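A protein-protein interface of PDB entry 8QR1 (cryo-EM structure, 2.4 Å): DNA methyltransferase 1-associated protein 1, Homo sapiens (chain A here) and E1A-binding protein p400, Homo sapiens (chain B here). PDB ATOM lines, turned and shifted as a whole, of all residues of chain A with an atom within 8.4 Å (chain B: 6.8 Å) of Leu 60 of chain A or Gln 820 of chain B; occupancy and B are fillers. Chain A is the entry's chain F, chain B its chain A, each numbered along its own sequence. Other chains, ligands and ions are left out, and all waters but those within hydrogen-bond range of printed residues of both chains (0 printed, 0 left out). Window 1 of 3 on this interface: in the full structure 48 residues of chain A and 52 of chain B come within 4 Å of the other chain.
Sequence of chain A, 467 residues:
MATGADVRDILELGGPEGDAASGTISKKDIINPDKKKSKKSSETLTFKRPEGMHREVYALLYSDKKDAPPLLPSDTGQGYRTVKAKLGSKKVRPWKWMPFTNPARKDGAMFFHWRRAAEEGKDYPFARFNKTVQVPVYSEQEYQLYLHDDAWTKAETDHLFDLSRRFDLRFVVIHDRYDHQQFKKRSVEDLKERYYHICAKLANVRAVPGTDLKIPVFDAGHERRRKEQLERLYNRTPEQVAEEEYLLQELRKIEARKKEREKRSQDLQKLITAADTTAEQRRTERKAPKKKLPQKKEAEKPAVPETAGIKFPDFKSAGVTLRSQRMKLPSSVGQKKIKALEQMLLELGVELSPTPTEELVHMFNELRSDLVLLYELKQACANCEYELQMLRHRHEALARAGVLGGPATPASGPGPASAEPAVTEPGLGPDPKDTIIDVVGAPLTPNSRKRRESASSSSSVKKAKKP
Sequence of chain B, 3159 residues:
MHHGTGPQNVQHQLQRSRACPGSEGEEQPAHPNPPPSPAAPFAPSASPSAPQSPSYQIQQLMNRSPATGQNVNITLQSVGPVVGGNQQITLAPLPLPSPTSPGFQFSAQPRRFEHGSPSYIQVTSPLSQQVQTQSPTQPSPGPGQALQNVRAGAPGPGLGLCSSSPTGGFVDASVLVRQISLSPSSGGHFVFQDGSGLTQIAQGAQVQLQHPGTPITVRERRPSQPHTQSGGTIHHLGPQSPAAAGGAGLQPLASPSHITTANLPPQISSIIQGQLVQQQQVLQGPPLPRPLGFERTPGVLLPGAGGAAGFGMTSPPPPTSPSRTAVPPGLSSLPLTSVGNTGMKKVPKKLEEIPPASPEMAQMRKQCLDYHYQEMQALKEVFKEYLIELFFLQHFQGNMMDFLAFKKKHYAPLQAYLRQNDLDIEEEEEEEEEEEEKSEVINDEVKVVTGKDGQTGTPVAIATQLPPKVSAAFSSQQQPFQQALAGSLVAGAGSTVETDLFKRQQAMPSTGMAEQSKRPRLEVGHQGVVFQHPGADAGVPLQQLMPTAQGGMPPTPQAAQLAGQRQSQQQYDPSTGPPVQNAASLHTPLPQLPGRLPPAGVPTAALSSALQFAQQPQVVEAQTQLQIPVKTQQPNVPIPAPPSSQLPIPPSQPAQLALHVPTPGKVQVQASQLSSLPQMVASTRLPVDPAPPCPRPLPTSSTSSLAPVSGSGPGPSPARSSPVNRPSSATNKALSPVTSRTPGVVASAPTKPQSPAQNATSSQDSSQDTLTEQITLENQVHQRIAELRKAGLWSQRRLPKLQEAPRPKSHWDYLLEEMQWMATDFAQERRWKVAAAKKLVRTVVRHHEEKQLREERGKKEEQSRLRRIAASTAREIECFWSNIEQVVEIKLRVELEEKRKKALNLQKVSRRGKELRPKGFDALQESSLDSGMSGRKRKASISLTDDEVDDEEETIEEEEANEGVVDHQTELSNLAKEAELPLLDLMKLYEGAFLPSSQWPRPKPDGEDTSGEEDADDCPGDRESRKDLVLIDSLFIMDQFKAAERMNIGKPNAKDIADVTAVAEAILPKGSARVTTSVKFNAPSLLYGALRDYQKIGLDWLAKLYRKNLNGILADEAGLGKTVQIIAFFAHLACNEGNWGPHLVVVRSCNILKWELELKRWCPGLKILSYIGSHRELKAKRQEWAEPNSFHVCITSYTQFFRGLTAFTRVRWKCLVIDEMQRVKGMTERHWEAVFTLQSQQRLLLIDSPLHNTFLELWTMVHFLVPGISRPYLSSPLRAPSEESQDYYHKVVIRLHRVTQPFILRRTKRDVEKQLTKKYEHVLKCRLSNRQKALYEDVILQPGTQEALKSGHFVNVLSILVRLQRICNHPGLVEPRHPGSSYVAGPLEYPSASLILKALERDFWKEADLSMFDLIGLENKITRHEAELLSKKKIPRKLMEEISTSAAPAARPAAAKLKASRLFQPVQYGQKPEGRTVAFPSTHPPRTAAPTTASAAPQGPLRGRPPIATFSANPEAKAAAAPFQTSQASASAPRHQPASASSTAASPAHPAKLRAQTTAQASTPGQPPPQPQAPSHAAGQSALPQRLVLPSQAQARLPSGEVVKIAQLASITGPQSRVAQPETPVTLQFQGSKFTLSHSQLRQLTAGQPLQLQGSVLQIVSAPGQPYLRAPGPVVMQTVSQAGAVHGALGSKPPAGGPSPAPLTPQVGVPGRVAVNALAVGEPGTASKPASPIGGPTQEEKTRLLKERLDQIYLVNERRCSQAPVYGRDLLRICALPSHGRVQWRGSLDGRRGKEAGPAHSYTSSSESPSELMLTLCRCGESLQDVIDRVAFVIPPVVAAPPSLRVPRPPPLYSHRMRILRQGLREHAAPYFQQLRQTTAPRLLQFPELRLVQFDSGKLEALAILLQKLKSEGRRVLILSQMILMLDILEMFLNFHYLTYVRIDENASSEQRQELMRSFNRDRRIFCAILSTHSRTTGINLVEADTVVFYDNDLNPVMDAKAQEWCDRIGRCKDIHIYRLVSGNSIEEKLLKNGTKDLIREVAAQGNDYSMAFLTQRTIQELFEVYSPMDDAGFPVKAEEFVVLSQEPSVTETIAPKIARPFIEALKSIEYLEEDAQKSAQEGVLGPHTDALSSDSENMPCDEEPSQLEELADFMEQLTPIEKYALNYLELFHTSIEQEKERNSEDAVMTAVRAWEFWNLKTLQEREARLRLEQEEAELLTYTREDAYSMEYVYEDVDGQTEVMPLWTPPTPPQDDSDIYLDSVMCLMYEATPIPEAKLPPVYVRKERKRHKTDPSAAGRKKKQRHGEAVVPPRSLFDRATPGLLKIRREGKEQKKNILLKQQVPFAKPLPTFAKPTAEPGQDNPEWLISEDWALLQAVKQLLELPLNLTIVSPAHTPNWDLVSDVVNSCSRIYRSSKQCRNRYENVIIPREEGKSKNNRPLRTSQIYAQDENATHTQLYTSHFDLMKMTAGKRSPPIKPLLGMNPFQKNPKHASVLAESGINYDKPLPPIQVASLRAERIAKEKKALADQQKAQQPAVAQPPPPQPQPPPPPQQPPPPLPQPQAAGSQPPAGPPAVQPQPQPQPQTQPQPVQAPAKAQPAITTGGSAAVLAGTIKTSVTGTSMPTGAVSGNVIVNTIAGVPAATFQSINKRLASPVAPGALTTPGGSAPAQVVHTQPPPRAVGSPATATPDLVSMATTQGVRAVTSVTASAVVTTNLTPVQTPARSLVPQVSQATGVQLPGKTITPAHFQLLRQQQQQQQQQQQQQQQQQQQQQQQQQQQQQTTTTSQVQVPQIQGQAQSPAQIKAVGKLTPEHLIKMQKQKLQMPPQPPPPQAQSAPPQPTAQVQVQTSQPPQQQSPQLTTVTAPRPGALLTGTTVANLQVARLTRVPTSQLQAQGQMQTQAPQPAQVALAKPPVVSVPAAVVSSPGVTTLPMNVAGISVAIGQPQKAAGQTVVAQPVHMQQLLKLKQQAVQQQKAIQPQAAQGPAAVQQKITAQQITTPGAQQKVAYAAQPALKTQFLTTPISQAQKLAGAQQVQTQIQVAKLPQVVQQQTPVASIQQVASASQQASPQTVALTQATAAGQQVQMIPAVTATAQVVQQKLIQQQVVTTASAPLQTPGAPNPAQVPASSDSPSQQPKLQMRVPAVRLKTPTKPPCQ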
ATOM      1  N   VAL A  57       4.574  23.813   6.875  1.00  0.00           N
ATOM      2  CA  VAL A  57       3.121  23.907   6.781  1.00  0.00           C
ATOM      3  C   VAL A  57       2.682  23.558   5.368  1.00  0.00           C
ATOM      4  O   VAL A  57       3.425  23.739   4.398  1.00  0.00           O
ATOM      5  CB  VAL A  57       2.602  25.308   7.184  1.00  0.00           C
ATOM      6  CG1 VAL A  57       3.039  25.644   8.594  1.00  0.00           C
ATOM      7  CG2 VAL A  57       3.068  26.380   6.225  1.00  0.00           C
ATOM      8  N   TYR A  58       1.449  23.059   5.265  1.00  0.00           N
ATOM      9  CA  TYR A  58       0.841  22.608   4.023  1.00  0.00           C
ATOM     10  C   TYR A  58      -0.526  23.257   3.880  1.00  0.00           C
ATOM     11  O   TYR A  58      -1.201  23.517   4.878  1.00  0.00           O
ATOM     12  CB  TYR A  58       0.669  21.087   3.991  1.00  0.00           C
ATOM     13  CG  TYR A  58       1.939  20.268   3.957  1.00  0.00           C
ATOM     14  CD1 TYR A  58       2.762  20.173   5.064  1.00  0.00           C
ATOM     15  CD2 TYR A  58       2.292  19.557   2.824  1.00  0.00           C
ATOM     16  CE1 TYR A  58       3.909  19.419   5.036  1.00  0.00           C
ATOM     17  CE2 TYR A  58       3.437  18.798   2.789  1.00  0.00           C
ATOM     18  CZ  TYR A  58       4.241  18.731   3.898  1.00  0.00           C
ATOM     19  OH  TYR A  58       5.387  17.975   3.871  1.00  0.00           O
ATOM     20  N   ALA A  59      -0.932  23.511   2.639  1.00  0.00           N
ATOM     21  CA  ALA A  59      -2.249  24.070   2.373  1.00  0.00           C
ATOM     22  C   ALA A  59      -2.538  23.982   0.885  1.00  0.00           C
ATOM     23  O   ALA A  59      -1.625  24.000   0.055  1.00  0.00           O
ATOM     24  CB  ALA A  59      -2.356  25.518   2.849  1.00  0.00           C
ATOM     25  N   LEU A  60      -3.826  23.886   0.560  1.00  0.00           N
ATOM     26  CA  LEU A  60      -4.260  23.835  -0.829  1.00  0.00           C
ATOM     27  C   LEU A  60      -4.363  25.237  -1.417  1.00  0.00           C
ATOM     28  O   LEU A  60      -3.574  25.601  -2.291  1.00  0.00           O
ATOM     29  CB  LEU A  60      -5.602  23.107  -0.931  1.00  0.00           C
ATOM     30  CG  LEU A  60      -6.237  22.925  -2.311  1.00  0.00           C
ATOM     31  CD1 LEU A  60      -5.325  22.164  -3.241  1.00  0.00           C
ATOM     32  CD2 LEU A  60      -7.554  22.211  -2.169  1.00  0.00           C
ATOM     33  N   LEU A  61      -5.302  26.040  -0.910  1.00  0.00           N
ATOM     34  CA  LEU A  61      -5.455  27.414  -1.378  1.00  0.00           C
ATOM     35  C   LEU A  61      -4.558  28.355  -0.586  1.00  0.00           C
ATOM     36  O   LEU A  61      -3.702  29.045  -1.151  1.00  0.00           O
ATOM     37  CB  LEU A  61      -6.918  27.851  -1.267  1.00  0.00           C
ATOM     38  CG  LEU A  61      -8.021  27.013  -1.913  1.00  0.00           C
ATOM     39  CD1 LEU A  61      -9.341  27.733  -1.799  1.00  0.00           C
ATOM     40  CD2 LEU A  61      -7.730  26.731  -3.358  1.00  0.00           C
ATOM     41  N   TYR A  62      -4.747  28.399   0.730  1.00  0.00           N
ATOM     42  CA  TYR A  62      -3.905  29.195   1.606  1.00  0.00           C
ATOM     43  C   TYR A  62      -4.044  28.656   3.020  1.00  0.00           C
ATOM     44  O   TYR A  62      -5.028  27.993   3.357  1.00  0.00           O
ATOM     45  CB  TYR A  62      -4.263  30.685   1.534  1.00  0.00           C
ATOM     46  CG  TYR A  62      -5.733  30.997   1.691  1.00  0.00           C
ATOM     47  CD1 TYR A  62      -6.309  31.125   2.945  1.00  0.00           C
ATOM     48  CD2 TYR A  62      -6.541  31.178   0.580  1.00  0.00           C
ATOM     49  CE1 TYR A  62      -7.647  31.413   3.088  1.00  0.00           C
ATOM     50  CE2 TYR A  62      -7.878  31.467   0.713  1.00  0.00           C
ATOM     51  CZ  TYR A  62      -8.427  31.583   1.969  1.00  0.00           C
ATOM     52  OH  TYR A  62      -9.762  31.873   2.108  1.00  0.00           O
ATOM     53  N   SER A  63      -3.038  28.947   3.843  1.00  0.00           N
ATOM     54  CA  SER A  63      -2.993  28.395   5.190  1.00  0.00           C
ATOM     55  C   SER A  63      -3.975  29.087   6.126  1.00  0.00           C
ATOM     56  O   SER A  63      -4.605  28.430   6.961  1.00  0.00           O
ATOM     57  CB  SER A  63      -1.576  28.502   5.746  1.00  0.00           C
ATOM     58  OG  SER A  63      -0.673  27.730   4.981  1.00  0.00           O
ATOM     59  N   LEU B 815      -8.414  17.089 -15.834  1.00  0.00           N
ATOM     60  CA  LEU B 815      -9.264  18.266 -15.697  1.00  0.00           C
ATOM     61  C   LEU B 815      -9.395  18.686 -14.239  1.00  0.00           C
ATOM     62  O   LEU B 815      -9.347  19.878 -13.925  1.00  0.00           O
ATOM     63  CB  LEU B 815     -10.640  17.989 -16.293  1.00  0.00           C
ATOM     64  CG  LEU B 815     -11.581  19.187 -16.372  1.00  0.00           C
ATOM     65  CD1 LEU B 815     -12.257  19.233 -17.715  1.00  0.00           C
ATOM     66  CD2 LEU B 815     -12.617  19.138 -15.278  1.00  0.00           C
ATOM     67  N   LEU B 816      -9.567  17.722 -13.337  1.00  0.00           N
ATOM     68  CA  LEU B 816      -9.676  18.048 -11.918  1.00  0.00           C
ATOM     69  C   LEU B 816      -8.368  18.600 -11.357  1.00  0.00           C
ATOM     70  O   LEU B 816      -8.387  19.507 -10.512  1.00  0.00           O
ATOM     71  CB  LEU B 816     -10.110  16.811 -11.138  1.00  0.00           C
ATOM     72  CG  LEU B 816     -11.517  16.285 -11.433  1.00  0.00           C
ATOM     73  CD1 LEU B 816     -11.707  14.912 -10.832  1.00  0.00           C
ATOM     74  CD2 LEU B 816     -12.579  17.224 -10.926  1.00  0.00           C
ATOM     75  N   GLU B 817      -7.230  18.066 -11.800  1.00  0.00           N
ATOM     76  CA  GLU B 817      -5.948  18.620 -11.369  1.00  0.00           C
ATOM     77  C   GLU B 817      -5.790  20.067 -11.830  1.00  0.00           C
ATOM     78  O   GLU B 817      -5.377  20.945 -11.051  1.00  0.00           O
ATOM     79  CB  GLU B 817      -4.809  17.755 -11.902  1.00  0.00           C
ATOM     80  CG  GLU B 817      -4.650  16.437 -11.177  1.00  0.00           C
ATOM     81  CD  GLU B 817      -3.648  15.519 -11.846  1.00  0.00           C
ATOM     82  OE1 GLU B 817      -2.838  16.013 -12.657  1.00  0.00           O
ATOM     83  OE2 GLU B 817      -3.671  14.304 -11.560  1.00  0.00           O
ATOM     84  N   GLU B 818      -6.140  20.337 -13.089  1.00  0.00           N
ATOM     85  CA  GLU B 818      -6.085  21.701 -13.597  1.00  0.00           C
ATOM     86  C   GLU B 818      -7.076  22.599 -12.868  1.00  0.00           C
ATOM     87  O   GLU B 818      -6.814  23.791 -12.677  1.00  0.00           O
ATOM     88  CB  GLU B 818      -6.357  21.708 -15.098  1.00  0.00           C
ATOM     89  CG  GLU B 818      -5.734  22.873 -15.830  1.00  0.00           C
ATOM     90  CD  GLU B 818      -6.317  23.070 -17.207  1.00  0.00           C
ATOM     91  OE1 GLU B 818      -6.794  22.079 -17.792  1.00  0.00           O
ATOM     92  OE2 GLU B 818      -6.288  24.211 -17.710  1.00  0.00           O
ATOM     93  N   MET B 819      -8.216  22.044 -12.455  1.00  0.00           N
ATOM     94  CA  MET B 819      -9.184  22.806 -11.675  1.00  0.00           C
ATOM     95  C   MET B 819      -8.593  23.234 -10.343  1.00  0.00           C
ATOM     96  O   MET B 819      -8.792  24.370  -9.903  1.00  0.00           O
ATOM     97  CB  MET B 819     -10.450  21.974 -11.462  1.00  0.00           C
ATOM     98  CG  MET B 819     -11.465  22.561 -10.485  1.00  0.00           C
ATOM     99  SD  MET B 819     -11.279  22.125  -8.735  1.00  0.00           S
ATOM    100  CE  MET B 819     -11.507  20.357  -8.758  1.00  0.00           C
ATOM    101  N   GLN B 820      -7.895  22.317  -9.667  1.00  0.00           N
ATOM    102  CA  GLN B 820      -7.255  22.656  -8.396  1.00  0.00           C
ATOM    103  C   GLN B 820      -6.244  23.778  -8.586  1.00  0.00           C
ATOM    104  O   GLN B 820      -6.226  24.764  -7.831  1.00  0.00           O
ATOM    105  CB  GLN B 820      -6.564  21.424  -7.818  1.00  0.00           C
ATOM    106  CG  GLN B 820      -7.484  20.330  -7.348  1.00  0.00           C
ATOM    107  CD  GLN B 820      -6.953  19.615  -6.123  1.00  0.00           C
ATOM    108  OE1 GLN B 820      -5.820  19.137  -6.115  1.00  0.00           O
ATOM    109  NE2 GLN B 820      -7.780  19.514  -5.090  1.00  0.00           N
ATOM    110  N   TRP B 821      -5.416  23.647  -9.625  1.00  0.00           N
ATOM    111  CA  TRP B 821      -4.396  24.650  -9.916  1.00  0.00           C
ATOM    112  C   TRP B 821      -5.021  26.015 -10.206  1.00  0.00           C
ATOM    113  O   TRP B 821      -4.591  27.046  -9.662  1.00  0.00           O
ATOM    114  CB  TRP B 821      -3.558  24.149 -11.093  1.00  0.00           C
ATOM    115  CG  TRP B 821      -2.560  25.092 -11.623  1.00  0.00           C
ATOM    116  CD1 TRP B 821      -1.324  25.342 -11.120  1.00  0.00           C
ATOM    117  CD2 TRP B 821      -2.691  25.901 -12.792  1.00  0.00           C
ATOM    118  NE1 TRP B 821      -0.678  26.268 -11.895  1.00  0.00           N
ATOM    119  CE2 TRP B 821      -1.499  26.627 -12.930  1.00  0.00           C
ATOM    120  CE3 TRP B 821      -3.704  26.086 -13.732  1.00  0.00           C
ATOM    121  CZ2 TRP B 821      -1.292  27.525 -13.965  1.00  0.00           C
ATOM    122  CZ3 TRP B 821      -3.498  26.976 -14.757  1.00  0.00           C
ATOM    123  CH2 TRP B 821      -2.302  27.685 -14.868  1.00  0.00           C
ATOM    124  N   MET B 822      -6.082  26.035 -11.012  1.00  0.00           N
ATOM    125  CA  MET B 822      -6.713  27.298 -11.367  1.00  0.00           C
ATOM    126  C   MET B 822      -7.449  27.911 -10.182  1.00  0.00           C
ATOM    127  O   MET B 822      -7.520  29.137 -10.059  1.00  0.00           O
ATOM    128  CB  MET B 822      -7.662  27.082 -12.544  1.00  0.00           C
ATOM    129  CG  MET B 822      -8.252  28.342 -13.142  1.00  0.00           C
ATOM    130  SD  MET B 822      -7.032  29.443 -13.861  1.00  0.00           S
ATOM    131  CE  MET B 822      -6.738  28.600 -15.401  1.00  0.00           C
ATOM    132  N   ALA B 823      -8.027  27.080  -9.315  1.00  0.00           N
ATOM    133  CA  ALA B 823      -8.695  27.605  -8.131  1.00  0.00           C
ATOM    134  C   ALA B 823      -7.707  28.289  -7.200  1.00  0.00           C
ATOM    135  O   ALA B 823      -7.997  29.361  -6.645  1.00  0.00           O
ATOM    136  CB  ALA B 823      -9.426  26.479  -7.409  1.00  0.00           C
ATOM    137  N   THR B 824      -6.524  27.686  -7.020  1.00  0.00           N
ATOM    138  CA  THR B 824      -5.487  28.360  -6.242  1.00  0.00           C
ATOM    139  C   THR B 824      -5.072  29.671  -6.888  1.00  0.00           C
ATOM    140  O   THR B 824      -4.869  30.669  -6.182  1.00  0.00           O
ATOM    141  CB  THR B 824      -4.258  27.473  -6.078  1.00  0.00           C
ATOM    142  OG1 THR B 824      -3.701  27.188  -7.363  1.00  0.00           O
ATOM    143  CG2 THR B 824      -4.614  26.190  -5.403  1.00  0.00           C
ATOM    144  N   ASP B 825      -4.946  29.685  -8.219  1.00  0.00           N
ATOM    145  CA  ASP B 825      -4.594  30.920  -8.915  1.00  0.00           C
ATOM    146  C   ASP B 825      -5.636  32.008  -8.686  1.00  0.00           C
ATOM    147  O   ASP B 825      -5.286  33.160  -8.402  1.00  0.00           O
ATOM    148  CB  ASP B 825      -4.424  30.648 -10.407  1.00  0.00           C
ATOM    149  CG  ASP B 825      -3.624  31.721 -11.109  1.00  0.00           C
ATOM    150  OD1 ASP B 825      -2.485  31.996 -10.678  1.00  0.00           O
ATOM    151  OD2 ASP B 825      -4.130  32.287 -12.098  1.00  0.00           O
ATOM    152  N   GLN B 828      -5.477  33.269  -4.870  1.00  0.00           N
ATOM    153  CA  GLN B 828      -4.291  34.046  -4.560  1.00  0.00           C
ATOM    154  C   GLN B 828      -4.257  35.360  -5.328  1.00  0.00           C
ATOM    155  O   GLN B 828      -3.807  36.375  -4.783  1.00  0.00           O
ATOM    156  CB  GLN B 828      -3.044  33.214  -4.850  1.00  0.00           C
ATOM    157  CG  GLN B 828      -2.860  32.024  -3.925  1.00  0.00           C
ATOM    158  CD  GLN B 828      -2.547  32.415  -2.500  1.00  0.00           C
ATOM    159  OE1 GLN B 828      -3.447  32.620  -1.689  1.00  0.00           O
ATOM    160  NE2 GLN B 828      -1.269  32.522  -2.187  1.00  0.00           N
ATOM    161  N   TRP B2248       4.895  23.862  -8.351  1.00  0.00           N
ATOM    162  CA  TRP B2248       3.564  23.402  -8.733  1.00  0.00           C
ATOM    163  C   TRP B2248       3.300  23.923 -10.138  1.00  0.00           C
ATOM    164  O   TRP B2248       3.131  25.126 -10.347  1.00  0.00           O
ATOM    165  CB  TRP B2248       2.530  23.896  -7.727  1.00  0.00           C
ATOM    166  CG  TRP B2248       1.110  23.385  -7.877  1.00  0.00           C
ATOM    167  CD1 TRP B2248       0.590  22.619  -8.885  1.00  0.00           C
ATOM    168  CD2 TRP B2248       0.036  23.614  -6.965  1.00  0.00           C
ATOM    169  NE1 TRP B2248      -0.733  22.367  -8.655  1.00  0.00           N
ATOM    170  CE2 TRP B2248      -1.099  22.966  -7.482  1.00  0.00           C
ATOM    171  CE3 TRP B2248      -0.077  24.308  -5.761  1.00  0.00           C
ATOM    172  CZ2 TRP B2248      -2.324  22.992  -6.836  1.00  0.00           C
ATOM    173  CZ3 TRP B2248      -1.292  24.330  -5.125  1.00  0.00           C
ATOM    174  CH2 TRP B2248      -2.399  23.678  -5.661  1.00  0.00           C
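Among the printed residues, merely in contact across the chains: Leu 60 of chain A with Gln 820 of chain B, Leu 60 of chain A with Thr 824 of chain B, Leu 60 of chain A with Trp 2248 of chain B, Leu 61 of chain A with Thr 824 of chain B, Leu 61 of chain A with Gln 828 of chain B and Tyr 62 of chain A with Gln 828 of chain B.
Ser 63 of chain A touches none of the printed residues of chain B. No residue of chain A comes within 4 Å of Met 819 of chain B. Printed residues of chain A within 4 Å of Gln 820 of chain B: Leu 60 (3.98 Å). Printed residues of chain A within 4 Å of Gln 828 of chain B: Leu 61 and Tyr 62. Printed residues of chain A within 4 Å of Trp 2248 of chain B: Leu 60. The nearest printed residue of chain A that does not touch Gln 820 of chain B is Leu 61 of chain A (5.1 Å). The nearest printed residue of chain A that does not touch Trp 2248 of chain B is Ala 59 of chain A (5.2 Å).
The backbone carbonyl oxygen (O) of Trp 821 of chain B is in hydrogen-bond range of the side-chain hydroxyl (OG1) of Thr 824 of chain B.
Of the 13 printed residues of chain B, 4 touch a printed residue of chain A. Hydrophobic or aromatic side chains of chain B within 4 Å of the printed part of chain A: Trp 2248. Among the printed residues, no Asp or Glu carboxylate lies within 4 Å of a Lys or Arg side-chain nitrogen of the other chain.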
